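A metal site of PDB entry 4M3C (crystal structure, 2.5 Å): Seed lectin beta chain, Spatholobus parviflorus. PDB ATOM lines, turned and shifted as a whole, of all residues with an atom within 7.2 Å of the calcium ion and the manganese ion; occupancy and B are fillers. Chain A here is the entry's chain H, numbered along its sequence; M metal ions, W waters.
Water W1 lies within hydrogen-bond range of OE1 of Glu 126 (2.6 Å) and O of Ile 150 (2.7 Å).
The manganese ion is bound by the side-chain carboxylate (OD1) of Asp 128 (1.9 Å).
A ring nitrogen (NE2) of His 142 binds the manganese ion (2.1 Å).
OE2 of Glu 126 is bound to the manganese ion, 2.1 Å away.
OD2 of Asp 137 binds the manganese ion (2.4 Å).
The manganese ion is bound by water W1, at 2.4 Å.
Four residues have an atom within 4 Å of the manganese ion: Glu 126, Asp 128, Asp 137 and His 142.
The nearest printed residue that does not touch the manganese ion is Ser 152 (4.1 Å).
N of Glu 126 lies within hydrogen-bond range of O of Gly 144 (2.9 Å).
A ring nitrogen (ND1) of His 142 sits at hydrogen-bond distance from the backbone carbonyl oxygen of Tyr 140.
The side-chain carboxylate of Glu 126 sits close to the side-chain hydroxyl of Ser 152, at 3.3 Å.
OD1 of Asn 132 binds the calcium ion (2.1 Å).
O of Tyr 130 is bound to the calcium ion.
The calcium ion is bound by water W2 (2.4 Å).
OD1 of Asp 137 is bound to the calcium ion, at 2.4 Å.
The calcium ion is bound by OD2 of Asp 128 (2.5 Å).
The calcium ion is bound by water W3 (2.5 Å).
The calcium ion is bound by OD1 of Asp 128, 2.8 Å away.
The calcium ion has seven donor atoms within binding distance.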
ATOM      1  N   ASP A  88      -7.450  23.719 -13.007  1.00  0.00           N
ATOM      2  CA  ASP A  88      -8.368  24.234 -14.018  1.00  0.00           C
ATOM      3  C   ASP A  88      -9.353  23.148 -14.442  1.00  0.00           C
ATOM      4  O   ASP A  88     -10.491  23.468 -14.858  1.00  0.00           O
ATOM      5  CB  ASP A  88      -7.598  24.693 -15.255  1.00  0.00           C
ATOM      6  CG  ASP A  88      -7.005  26.069 -15.086  1.00  0.00           C
ATOM      7  OD1 ASP A  88      -7.567  27.041 -15.635  1.00  0.00           O
ATOM      8  OD2 ASP A  88      -5.973  26.157 -14.401  1.00  0.00           O
ATOM      9  N   GLY A  89      -8.913  21.883 -14.302  1.00  0.00           N
ATOM     10  CA  GLY A  89      -9.765  20.762 -14.614  1.00  0.00           C
ATOM     11  C   GLY A  89      -9.105  19.512 -15.128  1.00  0.00           C
ATOM     12  O   GLY A  89      -7.893  19.449 -15.226  1.00  0.00           O
ATOM     13  N   GLY A 105      -3.004  25.513 -17.866  1.00  0.00           N
ATOM     14  CA  GLY A 105      -4.119  26.367 -17.394  1.00  0.00           C
ATOM     15  C   GLY A 105      -5.463  25.860 -17.921  1.00  0.00           C
ATOM     16  O   GLY A 105      -5.683  24.662 -18.059  1.00  0.00           O
ATOM     17  N   GLY A 106      -6.367  26.775 -18.245  1.00  0.00           N
ATOM     18  CA  GLY A 106      -7.659  26.447 -18.881  1.00  0.00           C
ATOM     19  C   GLY A 106      -7.612  25.832 -20.271  1.00  0.00           C
ATOM     20  O   GLY A 106      -8.654  25.613 -20.898  1.00  0.00           O
ATOM     21  N   PHE A 107      -6.425  25.521 -20.774  1.00  0.00           N
ATOM     22  CA  PHE A 107      -6.306  24.844 -22.066  1.00  0.00           C
ATOM     23  C   PHE A 107      -6.420  23.354 -21.834  1.00  0.00           C
ATOM     24  O   PHE A 107      -6.673  22.599 -22.770  1.00  0.00           O
ATOM     25  CB  PHE A 107      -4.965  25.198 -22.738  1.00  0.00           C
ATOM     26  CG  PHE A 107      -4.832  26.647 -23.046  1.00  0.00           C
ATOM     27  CD1 PHE A 107      -5.407  27.187 -24.177  1.00  0.00           C
ATOM     28  CD2 PHE A 107      -4.187  27.486 -22.168  1.00  0.00           C
ATOM     29  CE1 PHE A 107      -5.305  28.532 -24.455  1.00  0.00           C
ATOM     30  CE2 PHE A 107      -4.076  28.842 -22.435  1.00  0.00           C
ATOM     31  CZ  PHE A 107      -4.641  29.371 -23.586  1.00  0.00           C
ATOM     32  N   LEU A 108      -6.205  22.935 -20.591  1.00  0.00           N
ATOM     33  CA  LEU A 108      -6.380  21.548 -20.169  1.00  0.00           C
ATOM     34  C   LEU A 108      -5.517  20.589 -20.952  1.00  0.00           C
ATOM     35  O   LEU A 108      -5.785  19.394 -20.978  1.00  0.00           O
ATOM     36  CB  LEU A 108      -7.884  21.103 -20.249  1.00  0.00           C
ATOM     37  CG  LEU A 108      -8.841  21.986 -19.445  1.00  0.00           C
ATOM     38  CD1 LEU A 108     -10.276  21.495 -19.523  1.00  0.00           C
ATOM     39  CD2 LEU A 108      -8.375  22.076 -18.005  1.00  0.00           C
ATOM     40  N   GLU A 126     -14.725  17.768 -20.921  1.00  0.00           N
ATOM     41  CA  GLU A 126     -14.047  18.492 -19.852  1.00  0.00           C
ATOM     42  C   GLU A 126     -14.833  18.558 -18.546  1.00  0.00           C
ATOM     43  O   GLU A 126     -16.064  18.645 -18.545  1.00  0.00           O
ATOM     44  CB  GLU A 126     -13.642  19.877 -20.319  1.00  0.00           C
ATOM     45  CG  GLU A 126     -14.790  20.836 -20.468  1.00  0.00           C
ATOM     46  CD  GLU A 126     -14.388  22.296 -20.711  1.00  0.00           C
ATOM     47  OE1 GLU A 126     -13.395  22.551 -21.471  1.00  0.00           O
ATOM     48  OE2 GLU A 126     -15.118  23.171 -20.155  1.00  0.00           O
ATOM     49  N   PHE A 127     -14.085  18.501 -17.438  1.00  0.00           N
ATOM     50  CA  PHE A 127     -14.615  18.655 -16.096  1.00  0.00           C
ATOM     51  C   PHE A 127     -13.863  19.856 -15.572  1.00  0.00           C
ATOM     52  O   PHE A 127     -12.704  19.767 -15.170  1.00  0.00           O
ATOM     53  CB  PHE A 127     -14.378  17.376 -15.286  1.00  0.00           C
ATOM     54  CG  PHE A 127     -15.111  16.195 -15.868  1.00  0.00           C
ATOM     55  CD1 PHE A 127     -16.417  15.920 -15.483  1.00  0.00           C
ATOM     56  CD2 PHE A 127     -14.536  15.433 -16.899  1.00  0.00           C
ATOM     57  CE1 PHE A 127     -17.118  14.881 -16.075  1.00  0.00           C
ATOM     58  CE2 PHE A 127     -15.227  14.380 -17.477  1.00  0.00           C
ATOM     59  CZ  PHE A 127     -16.528  14.109 -17.071  1.00  0.00           C
ATOM     60  N   ASP A 128     -14.539  20.988 -15.600  1.00  0.00           N
ATOM     61  CA  ASP A 128     -13.852  22.268 -15.690  1.00  0.00           C
ATOM     62  C   ASP A 128     -14.101  23.151 -14.454  1.00  0.00           C
ATOM     63  O   ASP A 128     -15.233  23.601 -14.230  1.00  0.00           O
ATOM     64  CB  ASP A 128     -14.287  22.978 -16.995  1.00  0.00           C
ATOM     65  CG  ASP A 128     -13.572  24.296 -17.233  1.00  0.00           C
ATOM     66  OD1 ASP A 128     -13.830  24.912 -18.303  1.00  0.00           O
ATOM     67  OD2 ASP A 128     -12.769  24.747 -16.383  1.00  0.00           O
ATOM     68  N   THR A 129     -13.035  23.427 -13.699  1.00  0.00           N
ATOM     69  CA  THR A 129     -13.190  23.889 -12.337  1.00  0.00           C
ATOM     70  C   THR A 129     -12.988  25.370 -12.070  1.00  0.00           C
ATOM     71  O   THR A 129     -13.163  25.805 -10.931  1.00  0.00           O
ATOM     72  CB  THR A 129     -12.236  23.180 -11.406  1.00  0.00           C
ATOM     73  OG1 THR A 129     -10.921  23.288 -11.952  1.00  0.00           O
ATOM     74  CG2 THR A 129     -12.704  21.680 -11.178  1.00  0.00           C
ATOM     75  N   TYR A 130     -12.642  26.104 -13.126  1.00  0.00           N
ATOM     76  CA  TYR A 130     -12.338  27.511 -13.059  1.00  0.00           C
ATOM     77  C   TYR A 130     -12.772  28.258 -14.342  1.00  0.00           C
ATOM     78  O   TYR A 130     -12.493  27.800 -15.477  1.00  0.00           O
ATOM     79  CB  TYR A 130     -10.841  27.696 -12.776  1.00  0.00           C
ATOM     80  CG  TYR A 130     -10.334  29.138 -12.889  1.00  0.00           C
ATOM     81  CD1 TYR A 130     -10.335  29.997 -11.791  1.00  0.00           C
ATOM     82  CD2 TYR A 130      -9.841  29.614 -14.101  1.00  0.00           C
ATOM     83  CE1 TYR A 130      -9.853  31.281 -11.903  1.00  0.00           C
ATOM     84  CE2 TYR A 130      -9.375  30.899 -14.228  1.00  0.00           C
ATOM     85  CZ  TYR A 130      -9.369  31.715 -13.133  1.00  0.00           C
ATOM     86  OH  TYR A 130      -8.898  33.009 -13.305  1.00  0.00           O
ATOM     87  N   GLU A 131     -13.435  29.388 -14.140  1.00  0.00           N
ATOM     88  CA  GLU A 131     -14.095  30.122 -15.205  1.00  0.00           C
ATOM     89  C   GLU A 131     -13.155  31.018 -15.982  1.00  0.00           C
ATOM     90  O   GLU A 131     -12.672  32.017 -15.451  1.00  0.00           O
ATOM     91  CB  GLU A 131     -15.204  30.987 -14.621  1.00  0.00           C
ATOM     92  CG  GLU A 131     -15.918  31.798 -15.697  1.00  0.00           C
ATOM     93  CD  GLU A 131     -16.906  32.783 -15.133  1.00  0.00           C
ATOM     94  OE1 GLU A 131     -16.703  33.226 -13.989  1.00  0.00           O
ATOM     95  OE2 GLU A 131     -17.873  33.140 -15.839  1.00  0.00           O
ATOM     96  N   ASN A 132     -12.933  30.672 -17.241  1.00  0.00           N
ATOM     97  CA  ASN A 132     -12.108  31.496 -18.133  1.00  0.00           C
ATOM     98  C   ASN A 132     -13.033  32.246 -19.055  1.00  0.00           C
ATOM     99  O   ASN A 132     -13.634  31.692 -19.976  1.00  0.00           O
ATOM    100  CB  ASN A 132     -11.109  30.656 -18.921  1.00  0.00           C
ATOM    101  CG  ASN A 132     -10.396  29.633 -18.071  1.00  0.00           C
ATOM    102  OD1 ASN A 132     -10.976  28.630 -17.682  1.00  0.00           O
ATOM    103  ND2 ASN A 132      -9.131  29.877 -17.771  1.00  0.00           N
ATOM    104  N   THR A 133     -13.189  33.528 -18.730  1.00  0.00           N
ATOM    105  CA  THR A 133     -14.127  34.409 -19.408  1.00  0.00           C
ATOM    106  C   THR A 133     -13.702  34.504 -20.885  1.00  0.00           C
ATOM    107  O   THR A 133     -14.519  34.483 -21.815  1.00  0.00           O
ATOM    108  CB  THR A 133     -14.199  35.765 -18.651  1.00  0.00           C
ATOM    109  OG1 THR A 133     -15.528  36.270 -18.720  1.00  0.00           O
ATOM    110  CG2 THR A 133     -13.177  36.828 -19.160  1.00  0.00           C
ATOM    111  N   PHE A 135     -12.841  32.125 -22.501  1.00  0.00           N
ATOM    112  CA  PHE A 135     -13.295  30.912 -23.203  1.00  0.00           C
ATOM    113  C   PHE A 135     -14.788  30.793 -23.369  1.00  0.00           C
ATOM    114  O   PHE A 135     -15.266  29.806 -23.977  1.00  0.00           O
ATOM    115  CB  PHE A 135     -12.762  29.605 -22.564  1.00  0.00           C
ATOM    116  CG  PHE A 135     -11.276  29.521 -22.517  1.00  0.00           C
ATOM    117  CD1 PHE A 135     -10.480  30.265 -23.407  1.00  0.00           C
ATOM    118  CD2 PHE A 135     -10.644  28.682 -21.604  1.00  0.00           C
ATOM    119  CE1 PHE A 135      -9.083  30.196 -23.363  1.00  0.00           C
ATOM    120  CE2 PHE A 135      -9.259  28.617 -21.553  1.00  0.00           C
ATOM    121  CZ  PHE A 135      -8.474  29.372 -22.424  1.00  0.00           C
ATOM    122  N   THR A 136     -15.527  31.767 -22.838  1.00  0.00           N
ATOM    123  CA  THR A 136     -16.991  31.749 -22.786  1.00  0.00           C
ATOM    124  C   THR A 136     -17.473  30.790 -21.665  1.00  0.00           C
ATOM    125  O   THR A 136     -18.656  30.412 -21.609  1.00  0.00           O
ATOM    126  CB  THR A 136     -17.702  31.488 -24.165  1.00  0.00           C
ATOM    127  OG1 THR A 136     -17.304  32.465 -25.155  1.00  0.00           O
ATOM    128  CG2 THR A 136     -19.245  31.606 -24.043  1.00  0.00           C
ATOM    129  N   ASP A 137     -16.558  30.432 -20.757  1.00  0.00           N
ATOM    130  CA  ASP A 137     -16.934  29.609 -19.600  1.00  0.00           C
ATOM    131  C   ASP A 137     -18.192  30.118 -18.867  1.00  0.00           C
ATOM    132  O   ASP A 137     -18.349  31.322 -18.630  1.00  0.00           O
ATOM    133  CB  ASP A 137     -15.771  29.448 -18.623  1.00  0.00           C
ATOM    134  CG  ASP A 137     -14.865  28.295 -18.971  1.00  0.00           C
ATOM    135  OD1 ASP A 137     -13.919  28.043 -18.205  1.00  0.00           O
ATOM    136  OD2 ASP A 137     -15.065  27.625 -20.010  1.00  0.00           O
ATOM    137  N   PRO A 138     -19.088  29.199 -18.509  1.00  0.00           N
ATOM    138  CA  PRO A 138     -20.246  29.533 -17.686  1.00  0.00           C
ATOM    139  C   PRO A 138     -19.785  30.024 -16.305  1.00  0.00           C
ATOM    140  O   PRO A 138     -18.680  29.708 -15.873  1.00  0.00           O
ATOM    141  CB  PRO A 138     -20.984  28.195 -17.556  1.00  0.00           C
ATOM    142  CG  PRO A 138     -19.901  27.185 -17.662  1.00  0.00           C
ATOM    143  CD  PRO A 138     -18.934  27.735 -18.679  1.00  0.00           C
ATOM    144  N   TYR A 140     -20.122  29.091 -13.541  1.00  0.00           N
ATOM    145  CA  TYR A 140     -20.047  28.043 -12.553  1.00  0.00           C
ATOM    146  C   TYR A 140     -19.172  26.890 -13.113  1.00  0.00           C
ATOM    147  O   TYR A 140     -18.874  26.863 -14.330  1.00  0.00           O
ATOM    148  CB  TYR A 140     -21.452  27.541 -12.174  1.00  0.00           C
ATOM    149  CG  TYR A 140     -22.359  27.428 -13.393  1.00  0.00           C
ATOM    150  CD1 TYR A 140     -22.114  26.465 -14.391  1.00  0.00           C
ATOM    151  CD2 TYR A 140     -23.445  28.309 -13.579  1.00  0.00           C
ATOM    152  CE1 TYR A 140     -22.930  26.351 -15.504  1.00  0.00           C
ATOM    153  CE2 TYR A 140     -24.267  28.222 -14.705  1.00  0.00           C
ATOM    154  CZ  TYR A 140     -24.004  27.231 -15.650  1.00  0.00           C
ATOM    155  OH  TYR A 140     -24.799  27.123 -16.760  1.00  0.00           O
ATOM    156  N   HIS A 142     -18.419  23.405 -14.586  1.00  0.00           N
ATOM    157  CA  HIS A 142     -19.260  22.725 -15.549  1.00  0.00           C
ATOM    158  C   HIS A 142     -18.627  21.532 -16.137  1.00  0.00           C
ATOM    159  O   HIS A 142     -17.423  21.345 -16.006  1.00  0.00           O
ATOM    160  CB  HIS A 142     -19.559  23.688 -16.687  1.00  0.00           C
ATOM    161  CG  HIS A 142     -18.338  24.425 -17.180  1.00  0.00           C
ATOM    162  ND1 HIS A 142     -17.728  25.338 -16.447  1.00  0.00           N
ATOM    163  CD2 HIS A 142     -17.639  24.349 -18.373  1.00  0.00           C
ATOM    164  CE1 HIS A 142     -16.668  25.819 -17.119  1.00  0.00           C
ATOM    165  NE2 HIS A 142     -16.628  25.206 -18.303  1.00  0.00           N
ATOM    166  N   ILE A 143     -19.459  20.729 -16.777  1.00  0.00           N
ATOM    167  CA  ILE A 143     -19.069  19.659 -17.698  1.00  0.00           C
ATOM    168  C   ILE A 143     -19.240  20.265 -19.101  1.00  0.00           C
ATOM    169  O   ILE A 143     -20.193  21.016 -19.324  1.00  0.00           O
ATOM    170  CB  ILE A 143     -19.955  18.424 -17.475  1.00  0.00           C
ATOM    171  CG1 ILE A 143     -19.722  17.860 -16.065  1.00  0.00           C
ATOM    172  CG2 ILE A 143     -19.611  17.316 -18.453  1.00  0.00           C
ATOM    173  CD1 ILE A 143     -20.801  16.911 -15.522  1.00  0.00           C
ATOM    174  N   GLY A 144     -18.325  19.972 -20.008  1.00  0.00           N
ATOM    175  CA  GLY A 144     -18.347  20.624 -21.341  1.00  0.00           C
ATOM    176  C   GLY A 144     -17.932  19.674 -22.442  1.00  0.00           C
ATOM    177  O   GLY A 144     -17.097  18.780 -22.195  1.00  0.00           O
ATOM    178  N   ASP A 146     -15.985  19.449 -25.864  1.00  0.00           N
ATOM    179  CA  ASP A 146     -14.944  20.248 -26.543  1.00  0.00           C
ATOM    180  C   ASP A 146     -14.631  19.616 -27.885  1.00  0.00           C
ATOM    181  O   ASP A 146     -14.100  18.477 -27.964  1.00  0.00           O
ATOM    182  CB  ASP A 146     -13.671  20.237 -25.720  1.00  0.00           C
ATOM    183  CG  ASP A 146     -13.780  21.042 -24.454  1.00  0.00           C
ATOM    184  OD1 ASP A 146     -14.824  21.733 -24.237  1.00  0.00           O
ATOM    185  OD2 ASP A 146     -12.798  20.966 -23.667  1.00  0.00           O
ATOM    186  N   ILE A 150     -11.505  24.820 -27.061  1.00  0.00           N
ATOM    187  CA  ILE A 150     -11.707  24.887 -25.616  1.00  0.00           C
ATOM    188  C   ILE A 150     -13.007  25.592 -25.272  1.00  0.00           C
ATOM    189  O   ILE A 150     -13.418  25.603 -24.111  1.00  0.00           O
ATOM    190  CB  ILE A 150     -10.532  25.635 -24.883  1.00  0.00           C
ATOM    191  CG1 ILE A 150     -10.592  25.382 -23.373  1.00  0.00           C
ATOM    192  CG2 ILE A 150     -10.564  27.147 -25.180  1.00  0.00           C
ATOM    193  CD1 ILE A 150     -10.246  23.958 -22.964  1.00  0.00           C
ATOM    194  N   SER A 151     -13.601  26.223 -26.281  1.00  0.00           N
ATOM    195  CA  SER A 151     -14.902  26.855 -26.171  1.00  0.00           C
ATOM    196  C   SER A 151     -15.989  25.800 -26.351  1.00  0.00           C
ATOM    197  O   SER A 151     -16.484  25.579 -27.453  1.00  0.00           O
ATOM    198  CB  SER A 151     -15.049  27.959 -27.191  1.00  0.00           C
ATOM    199  OG  SER A 151     -14.696  29.193 -26.596  1.00  0.00           O
ATOM    200  N   SER A 152     -16.329  25.153 -25.252  1.00  0.00           N
ATOM    201  CA  SER A 152     -17.312  24.069 -25.250  1.00  0.00           C
ATOM    202  C   SER A 152     -18.491  24.335 -26.191  1.00  0.00           C
ATOM    203  O   SER A 152     -18.984  25.453 -26.246  1.00  0.00           O
ATOM    204  CB  SER A 152     -17.811  23.856 -23.829  1.00  0.00           C
ATOM    205  OG  SER A 152     -16.721  23.497 -22.986  1.00  0.00           O
ATOM    206  N   THR A 155     -22.512  22.866 -22.330  1.00  0.00           N
ATOM    207  CA  THR A 155     -22.074  22.635 -20.965  1.00  0.00           C
ATOM    208  C   THR A 155     -23.297  22.410 -20.040  1.00  0.00           C
ATOM    209  O   THR A 155     -24.448  22.680 -20.430  1.00  0.00           O
ATOM    210  CB  THR A 155     -21.396  23.874 -20.432  1.00  0.00           C
ATOM    211  OG1 THR A 155     -22.377  24.918 -20.429  1.00  0.00           O
ATOM    212  CG2 THR A 155     -20.166  24.344 -21.282  1.00  0.00           C
HETATM  213 CA    CA M   1     -11.927  26.818 -17.530  1.00  0.00          CA
HETATM  214 MN    MN M   2     -15.061  25.263 -19.727  1.00  0.00          MN
HETATM  215  O   HOH W   1     -13.315  25.166 -21.418  1.00  0.00           O
HETATM  216  O   HOH W   2     -11.127  26.187 -19.727  1.00  0.00           O
HETATM  217  O   HOH W   3      -9.974  25.596 -16.489  1.00  0.00           O
